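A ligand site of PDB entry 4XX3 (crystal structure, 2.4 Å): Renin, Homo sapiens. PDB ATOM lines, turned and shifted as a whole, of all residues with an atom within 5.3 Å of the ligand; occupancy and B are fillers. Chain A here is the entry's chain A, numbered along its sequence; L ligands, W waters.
An oxygen (O1) of the ligand sits at hydrogen-bond distance from the backbone NH (N) of Thr 85 (3.4 Å). The backbone carbonyl oxygen of Gly 228 lies within hydrogen-bond range of a nitrogen (N4) of the ligand (2.8 Å). The side-chain hydroxyl of Thr 85 lies within hydrogen-bond range of an oxygen (O1) of the ligand. OG of Ser 230 lies close to O2 of the ligand (3.3 Å). A nitrogen (N1) of the ligand lies within hydrogen-bond range of the side-chain carboxylate of Asp 38 (2.8 Å). The side-chain carboxylate of Asp 226 lies within hydrogen-bond range of a nitrogen (N3) of the ligand (2.7 Å). The backbone NH (N) of Ser 84 is in hydrogen-bond range of an oxygen (O1) of the ligand.
Water W2 bridges OG of Ser 230 (3.3 Å) and O2 of the ligand (3.3 Å).
Thr 18 touches the ligand. Gln 19 touches the ligand (CA to C4, 3.6 Å). Tyr 20 touches the ligand. Val 36 touches the ligand. CA of Gly 40 touches N3 of the ligand, at 3.9 Å. Tyr 83 touches the ligand. Phe 124 touches the ligand. CG2 of Val 127 touches C21 of the ligand, at 3.98 Å. Thr 227 touches the ligand. Ala 229 touches the ligand (C to C3, 3.5 Å). CE1 of His 301 touches C12 of the ligand, 3.9 Å away. Hydrophobic or aromatic side chains within 4 Å of the ligand: Val 36, Tyr 83, Phe 124, Val 127, Ala 229 and His 301. Of the 23 residues printed, 17 come within 4 Å of the ligand.
O of Ala 229 sits at hydrogen-bond distance from N of Ala 317, at 2.8 Å. N of Val 127 sits at hydrogen-bond distance from O of Trp 45 (2.9 Å). The side-chain hydroxyl of Tyr 83 sits at hydrogen-bond distance from the indole nitrogen of Trp 45 (2.8 Å). The backbone NH (N) of Ala 317 lies close to the backbone carbonyl oxygen (O) of Ser 230, at 3.4 Å. N of Gly 228 lies close to OD1 of Asp 38. The side-chain carboxylate (OD1) of Asp 38 sits at hydrogen-bond distance from the backbone NH (N) of Gly 40, 3.2 Å away. The backbone carbonyl oxygen (O) of Thr 227 sits at hydrogen-bond distance from the side-chain hydroxyl (OH) of Tyr 162 (2.7 Å). OD1 of Asp 226 is in hydrogen-bond range of N of Gly 228, 3.2 Å away.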
ATOM      1  N   THR A  18       8.488  21.265  29.279  1.00  0.00           N
ATOM      2  CA  THR A  18       8.326  21.085  27.836  1.00  0.00           C
ATOM      3  C   THR A  18       9.511  21.591  27.025  1.00  0.00           C
ATOM      4  O   THR A  18       9.617  21.216  25.870  1.00  0.00           O
ATOM      5  CB  THR A  18       6.994  21.707  27.332  1.00  0.00           C
ATOM      6  OG1 THR A  18       6.938  23.090  27.668  1.00  0.00           O
ATOM      7  CG2 THR A  18       5.768  21.018  27.858  1.00  0.00           C
ATOM      8  N   GLN A  19      10.336  22.500  27.584  1.00  0.00           N
ATOM      9  CA  GLN A  19      11.495  23.032  26.845  1.00  0.00           C
ATOM     10  C   GLN A  19      12.679  23.067  27.755  1.00  0.00           C
ATOM     11  O   GLN A  19      12.568  23.561  28.878  1.00  0.00           O
ATOM     12  CB  GLN A  19      11.225  24.440  26.264  1.00  0.00           C
ATOM     13  CG  GLN A  19      10.038  24.523  25.276  1.00  0.00           C
ATOM     14  CD  GLN A  19       9.691  25.918  24.871  1.00  0.00           C
ATOM     15  OE1 GLN A  19      10.564  26.714  24.512  1.00  0.00           O
ATOM     16  NE2 GLN A  19       8.423  26.251  24.870  1.00  0.00           N
ATOM     17  N   TYR A  20      13.791  22.455  27.316  1.00  0.00           N
ATOM     18  CA  TYR A  20      15.035  22.401  28.077  1.00  0.00           C
ATOM     19  C   TYR A  20      16.068  22.998  27.165  1.00  0.00           C
ATOM     20  O   TYR A  20      16.186  22.574  26.023  1.00  0.00           O
ATOM     21  CB  TYR A  20      15.408  20.964  28.465  1.00  0.00           C
ATOM     22  CG  TYR A  20      14.455  20.310  29.428  1.00  0.00           C
ATOM     23  CD1 TYR A  20      13.263  19.743  28.987  1.00  0.00           C
ATOM     24  CD2 TYR A  20      14.757  20.216  30.787  1.00  0.00           C
ATOM     25  CE1 TYR A  20      12.368  19.157  29.875  1.00  0.00           C
ATOM     26  CE2 TYR A  20      13.883  19.589  31.682  1.00  0.00           C
ATOM     27  CZ  TYR A  20      12.688  19.079  31.221  1.00  0.00           C
ATOM     28  OH  TYR A  20      11.814  18.459  32.066  1.00  0.00           O
ATOM     29  N   VAL A  36      18.282  24.511  22.235  1.00  0.00           N
ATOM     30  CA  VAL A  36      17.855  23.151  22.540  1.00  0.00           C
ATOM     31  C   VAL A  36      18.988  22.240  22.033  1.00  0.00           C
ATOM     32  O   VAL A  36      19.388  22.354  20.864  1.00  0.00           O
ATOM     33  CB  VAL A  36      16.527  22.792  21.811  1.00  0.00           C
ATOM     34  CG1 VAL A  36      16.126  21.322  22.055  1.00  0.00           C
ATOM     35  CG2 VAL A  36      15.403  23.724  22.210  1.00  0.00           C
ATOM     36  N   ASP A  38      19.513  18.992  20.729  1.00  0.00           N
ATOM     37  CA  ASP A  38      18.533  18.134  20.058  1.00  0.00           C
ATOM     38  C   ASP A  38      19.071  16.891  19.316  1.00  0.00           C
ATOM     39  O   ASP A  38      19.654  17.016  18.243  1.00  0.00           O
ATOM     40  CB  ASP A  38      17.766  19.054  19.088  1.00  0.00           C
ATOM     41  CG  ASP A  38      16.632  18.435  18.336  1.00  0.00           C
ATOM     42  OD1 ASP A  38      15.989  17.525  18.887  1.00  0.00           O
ATOM     43  OD2 ASP A  38      16.347  18.887  17.227  1.00  0.00           O
ATOM     44  N   GLY A  40      17.188  14.733  17.846  1.00  0.00           N
ATOM     45  CA  GLY A  40      16.301  14.550  16.700  1.00  0.00           C
ATOM     46  C   GLY A  40      16.576  15.419  15.490  1.00  0.00           C
ATOM     47  O   GLY A  40      15.736  15.507  14.601  1.00  0.00           O
ATOM     48  N   SER A  41      17.724  16.102  15.442  1.00  0.00           N
ATOM     49  CA  SER A  41      18.136  16.955  14.305  1.00  0.00           C
ATOM     50  C   SER A  41      19.669  17.058  14.306  1.00  0.00           C
ATOM     51  O   SER A  41      20.285  16.715  15.329  1.00  0.00           O
ATOM     52  CB  SER A  41      17.469  18.335  14.340  1.00  0.00           C
ATOM     53  OG  SER A  41      18.081  19.219  15.262  1.00  0.00           O
ATOM     54  N   TRP A  45      21.431  26.119  14.336  1.00  0.00           N
ATOM     55  CA  TRP A  45      20.831  27.332  13.808  1.00  0.00           C
ATOM     56  C   TRP A  45      20.413  28.256  14.928  1.00  0.00           C
ATOM     57  O   TRP A  45      20.039  27.789  16.011  1.00  0.00           O
ATOM     58  CB  TRP A  45      19.668  27.066  12.826  1.00  0.00           C
ATOM     59  CG  TRP A  45      18.412  26.510  13.435  1.00  0.00           C
ATOM     60  CD1 TRP A  45      18.016  25.203  13.433  1.00  0.00           C
ATOM     61  CD2 TRP A  45      17.323  27.255  14.027  1.00  0.00           C
ATOM     62  NE1 TRP A  45      16.765  25.085  14.025  1.00  0.00           N
ATOM     63  CE2 TRP A  45      16.323  26.330  14.381  1.00  0.00           C
ATOM     64  CE3 TRP A  45      17.123  28.627  14.306  1.00  0.00           C
ATOM     65  CZ2 TRP A  45      15.130  26.714  15.002  1.00  0.00           C
ATOM     66  CZ3 TRP A  45      15.928  29.007  14.918  1.00  0.00           C
ATOM     67  CH2 TRP A  45      14.957  28.059  15.268  1.00  0.00           C
ATOM     68  N   TYR A  83      10.956  20.519   9.778  1.00  0.00           N
ATOM     69  CA  TYR A  83      10.748  19.711  10.963  1.00  0.00           C
ATOM     70  C   TYR A  83       9.289  19.298  11.053  1.00  0.00           C
ATOM     71  O   TYR A  83       8.432  19.847  10.338  1.00  0.00           O
ATOM     72  CB  TYR A  83      11.095  20.516  12.244  1.00  0.00           C
ATOM     73  CG  TYR A  83      12.510  21.063  12.321  1.00  0.00           C
ATOM     74  CD1 TYR A  83      13.616  20.224  12.282  1.00  0.00           C
ATOM     75  CD2 TYR A  83      12.738  22.417  12.601  1.00  0.00           C
ATOM     76  CE1 TYR A  83      14.908  20.721  12.414  1.00  0.00           C
ATOM     77  CE2 TYR A  83      14.029  22.923  12.727  1.00  0.00           C
ATOM     78  CZ  TYR A  83      15.108  22.074  12.654  1.00  0.00           C
ATOM     79  OH  TYR A  83      16.395  22.550  12.810  1.00  0.00           O
ATOM     80  N   SER A  84       8.981  18.398  12.006  1.00  0.00           N
ATOM     81  CA  SER A  84       7.644  17.918  12.308  1.00  0.00           C
ATOM     82  C   SER A  84       6.739  19.026  12.864  1.00  0.00           C
ATOM     83  O   SER A  84       5.520  18.954  12.744  1.00  0.00           O
ATOM     84  CB  SER A  84       7.740  16.775  13.314  1.00  0.00           C
ATOM     85  OG  SER A  84       8.640  15.804  12.820  1.00  0.00           O
ATOM     86  N   THR A  85       7.334  20.010  13.535  1.00  0.00           N
ATOM     87  CA  THR A  85       6.599  21.111  14.176  1.00  0.00           C
ATOM     88  C   THR A  85       6.478  22.363  13.289  1.00  0.00           C
ATOM     89  O   THR A  85       5.715  23.261  13.607  1.00  0.00           O
ATOM     90  CB  THR A  85       7.227  21.447  15.536  1.00  0.00           C
ATOM     91  OG1 THR A  85       8.632  21.685  15.346  1.00  0.00           O
ATOM     92  CG2 THR A  85       7.009  20.370  16.548  1.00  0.00           C
ATOM     93  N   PHE A 119       7.347  29.087  16.786  1.00  0.00           N
ATOM     94  CA  PHE A 119       8.471  29.809  17.375  1.00  0.00           C
ATOM     95  C   PHE A 119       8.102  30.987  18.305  1.00  0.00           C
ATOM     96  O   PHE A 119       8.963  31.342  19.101  1.00  0.00           O
ATOM     97  CB  PHE A 119       9.487  30.211  16.297  1.00  0.00           C
ATOM     98  CG  PHE A 119      10.052  28.944  15.693  1.00  0.00           C
ATOM     99  CD1 PHE A 119      10.917  28.132  16.428  1.00  0.00           C
ATOM    100  CD2 PHE A 119       9.620  28.486  14.454  1.00  0.00           C
ATOM    101  CE1 PHE A 119      11.397  26.932  15.898  1.00  0.00           C
ATOM    102  CE2 PHE A 119      10.091  27.268  13.936  1.00  0.00           C
ATOM    103  CZ  PHE A 119      10.967  26.501  14.666  1.00  0.00           C
ATOM    104  N   PHE A 124      13.562  29.276  23.874  1.00  0.00           N
ATOM    105  CA  PHE A 124      14.898  29.193  23.321  1.00  0.00           C
ATOM    106  C   PHE A 124      14.916  30.031  22.054  1.00  0.00           C
ATOM    107  O   PHE A 124      13.853  30.306  21.457  1.00  0.00           O
ATOM    108  CB  PHE A 124      15.238  27.713  22.991  1.00  0.00           C
ATOM    109  CG  PHE A 124      14.246  26.992  22.092  1.00  0.00           C
ATOM    110  CD1 PHE A 124      13.164  26.305  22.621  1.00  0.00           C
ATOM    111  CD2 PHE A 124      14.416  26.977  20.707  1.00  0.00           C
ATOM    112  CE1 PHE A 124      12.249  25.640  21.791  1.00  0.00           C
ATOM    113  CE2 PHE A 124      13.519  26.297  19.869  1.00  0.00           C
ATOM    114  CZ  PHE A 124      12.441  25.620  20.415  1.00  0.00           C
ATOM    115  N   VAL A 127      18.638  26.090  17.852  1.00  0.00           N
ATOM    116  CA  VAL A 127      18.820  24.655  18.046  1.00  0.00           C
ATOM    117  C   VAL A 127      20.248  24.196  17.792  1.00  0.00           C
ATOM    118  O   VAL A 127      20.873  24.644  16.841  1.00  0.00           O
ATOM    119  CB  VAL A 127      17.782  23.847  17.183  1.00  0.00           C
ATOM    120  CG1 VAL A 127      18.042  22.332  17.219  1.00  0.00           C
ATOM    121  CG2 VAL A 127      16.332  24.153  17.599  1.00  0.00           C
ATOM    122  N   TYR A 162      17.279  15.490  32.568  1.00  0.00           N
ATOM    123  CA  TYR A 162      16.159  16.433  32.527  1.00  0.00           C
ATOM    124  C   TYR A 162      15.437  16.341  33.870  1.00  0.00           C
ATOM    125  O   TYR A 162      14.982  15.277  34.257  1.00  0.00           O
ATOM    126  CB  TYR A 162      15.192  16.092  31.359  1.00  0.00           C
ATOM    127  CG  TYR A 162      15.579  16.594  29.984  1.00  0.00           C
ATOM    128  CD1 TYR A 162      16.692  17.405  29.799  1.00  0.00           C
ATOM    129  CD2 TYR A 162      14.808  16.289  28.870  1.00  0.00           C
ATOM    130  CE1 TYR A 162      17.049  17.872  28.531  1.00  0.00           C
ATOM    131  CE2 TYR A 162      15.126  16.780  27.609  1.00  0.00           C
ATOM    132  CZ  TYR A 162      16.242  17.578  27.443  1.00  0.00           C
ATOM    133  OH  TYR A 162      16.550  18.069  26.184  1.00  0.00           O
ATOM    134  N   ASP A 226      14.578  11.299  21.368  1.00  0.00           N
ATOM    135  CA  ASP A 226      14.592  12.713  20.981  1.00  0.00           C
ATOM    136  C   ASP A 226      14.611  13.696  22.137  1.00  0.00           C
ATOM    137  O   ASP A 226      13.589  13.948  22.761  1.00  0.00           O
ATOM    138  CB  ASP A 226      13.396  12.985  20.027  1.00  0.00           C
ATOM    139  CG  ASP A 226      13.447  14.258  19.232  1.00  0.00           C
ATOM    140  OD1 ASP A 226      14.439  15.005  19.367  1.00  0.00           O
ATOM    141  OD2 ASP A 226      12.490  14.523  18.454  1.00  0.00           O
ATOM    142  N   THR A 227      15.775  14.320  22.376  1.00  0.00           N
ATOM    143  CA  THR A 227      15.970  15.306  23.446  1.00  0.00           C
ATOM    144  C   THR A 227      15.242  16.640  23.180  1.00  0.00           C
ATOM    145  O   THR A 227      14.937  17.383  24.121  1.00  0.00           O
ATOM    146  CB  THR A 227      17.454  15.482  23.755  1.00  0.00           C
ATOM    147  OG1 THR A 227      18.121  15.913  22.559  1.00  0.00           O
ATOM    148  CG2 THR A 227      18.083  14.210  24.275  1.00  0.00           C
ATOM    149  N   GLY A 228      14.951  16.900  21.912  1.00  0.00           N
ATOM    150  CA  GLY A 228      14.243  18.086  21.457  1.00  0.00           C
ATOM    151  C   GLY A 228      12.746  17.933  21.337  1.00  0.00           C
ATOM    152  O   GLY A 228      12.066  18.869  20.902  1.00  0.00           O
ATOM    153  N   ALA A 229      12.199  16.785  21.734  1.00  0.00           N
ATOM    154  CA  ALA A 229      10.754  16.560  21.726  1.00  0.00           C
ATOM    155  C   ALA A 229      10.270  16.613  23.168  1.00  0.00           C
ATOM    156  O   ALA A 229      10.938  16.098  24.057  1.00  0.00           O
ATOM    157  CB  ALA A 229      10.458  15.208  21.108  1.00  0.00           C
ATOM    158  N   SER A 230       9.162  17.306  23.420  1.00  0.00           N
ATOM    159  CA  SER A 230       8.623  17.459  24.782  1.00  0.00           C
ATOM    160  C   SER A 230       8.010  16.198  25.316  1.00  0.00           C
ATOM    161  O   SER A 230       8.128  15.873  26.495  1.00  0.00           O
ATOM    162  CB  SER A 230       7.553  18.552  24.820  1.00  0.00           C
ATOM    163  OG  SER A 230       7.998  19.765  24.268  1.00  0.00           O
ATOM    164  N   HIS A 301       1.449  12.332  22.938  1.00  0.00           N
ATOM    165  CA  HIS A 301       0.648  12.801  21.799  1.00  0.00           C
ATOM    166  C   HIS A 301       0.921  11.967  20.554  1.00  0.00           C
ATOM    167  O   HIS A 301       1.739  11.049  20.563  1.00  0.00           O
ATOM    168  CB  HIS A 301       0.853  14.313  21.538  1.00  0.00           C
ATOM    169  CG  HIS A 301       2.208  14.715  21.031  1.00  0.00           C
ATOM    170  ND1 HIS A 301       2.380  15.869  20.290  1.00  0.00           N
ATOM    171  CD2 HIS A 301       3.423  14.127  21.200  1.00  0.00           C
ATOM    172  CE1 HIS A 301       3.681  15.967  20.050  1.00  0.00           C
ATOM    173  NE2 HIS A 301       4.342  14.931  20.557  1.00  0.00           N
ATOM    174  N   MET A 303       2.181  11.841  16.588  1.00  0.00           N
ATOM    175  CA  MET A 303       3.097  12.516  15.691  1.00  0.00           C
ATOM    176  C   MET A 303       3.453  11.494  14.629  1.00  0.00           C
ATOM    177  O   MET A 303       4.064  10.480  14.936  1.00  0.00           O
ATOM    178  CB  MET A 303       4.340  13.002  16.495  1.00  0.00           C
ATOM    179  CG  MET A 303       5.215  14.056  15.813  1.00  0.00           C
ATOM    180  SD  MET A 303       4.566  15.752  15.546  1.00  0.00           S
ATOM    181  CE  MET A 303       3.495  15.964  16.895  1.00  0.00           C
ATOM    182  N   ALA A 317      11.214  14.357  26.278  1.00  0.00           N
ATOM    183  CA  ALA A 317      11.461  14.797  27.661  1.00  0.00           C
ATOM    184  C   ALA A 317      10.676  14.002  28.714  1.00  0.00           C
ATOM    185  O   ALA A 317      11.242  13.734  29.777  1.00  0.00           O
ATOM    186  CB  ALA A 317      11.219  16.294  27.819  1.00  0.00           C
HETATM  187  C1  LIG L   1      13.384  20.388  24.754  1.00  0.00           C
HETATM  188  C2  LIG L   1      12.314  19.542  24.598  1.00  0.00           C
HETATM  189  C3  LIG L   1      11.265  19.890  23.757  1.00  0.00           C
HETATM  190  C4  LIG L   1      13.375  21.590  24.070  1.00  0.00           C
HETATM  191  C5  LIG L   1      12.326  21.930  23.234  1.00  0.00           C
HETATM  192  C6  LIG L   1      11.242  21.083  23.058  1.00  0.00           C
HETATM  193  C7  LIG L   1      10.072  21.475  22.171  1.00  0.00           C
HETATM  194  C8  LIG L   1       9.421  17.595  18.083  1.00  0.00           C
HETATM  195  C9  LIG L   1       9.540  18.675  18.964  1.00  0.00           C
HETATM  196  C10 LIG L   1       8.470  19.074  19.738  1.00  0.00           C
HETATM  197  C11 LIG L   1       7.274  18.390  19.646  1.00  0.00           C
HETATM  198  C12 LIG L   1       7.146  17.324  18.771  1.00  0.00           C
HETATM  199  C13 LIG L   1       8.215  16.933  17.992  1.00  0.00           C
HETATM  200  C14 LIG L   1       8.553  20.212  20.687  1.00  0.00           C
HETATM  201  N1  LIG L   1      13.575  19.223  17.205  1.00  0.00           N
HETATM  202  C15 LIG L   1      13.043  20.459  16.708  1.00  0.00           C
HETATM  203  C16 LIG L   1      12.059  20.130  15.607  1.00  0.00           C
HETATM  204  C17 LIG L   1      11.081  19.018  15.887  1.00  0.00           C
HETATM  205  N2  LIG L   1      11.496  18.096  16.828  1.00  0.00           N
HETATM  206  C18 LIG L   1      12.841  18.051  17.234  1.00  0.00           C
HETATM  207  N3  LIG L   1      13.379  16.933  17.592  1.00  0.00           N
HETATM  208  O1  LIG L   1      10.004  18.967  15.304  1.00  0.00           O
HETATM  209  C19 LIG L   1      10.549  17.098  17.248  1.00  0.00           C
HETATM  210  C20 LIG L   1      12.380  21.287  17.840  1.00  0.00           C
HETATM  211  C21 LIG L   1      14.209  21.169  16.042  1.00  0.00           C
HETATM  212  C22 LIG L   1      13.208  21.468  19.094  1.00  0.00           C
HETATM  213  C23 LIG L   1      11.807  22.633  17.383  1.00  0.00           C
HETATM  214  O2  LIG L   1       7.505  20.684  21.110  1.00  0.00           O
HETATM  215  N4  LIG L   1       9.826  20.613  21.041  1.00  0.00           N
HETATM  216  O   HOH W   1       6.443  17.220  22.187  1.00  0.00           O
HETATM  217  O   HOH W   2       5.495  21.747  23.532  1.00  0.00           O
HETATM  218  O   HOH W   3       7.737  13.605  18.306  1.00  0.00           O
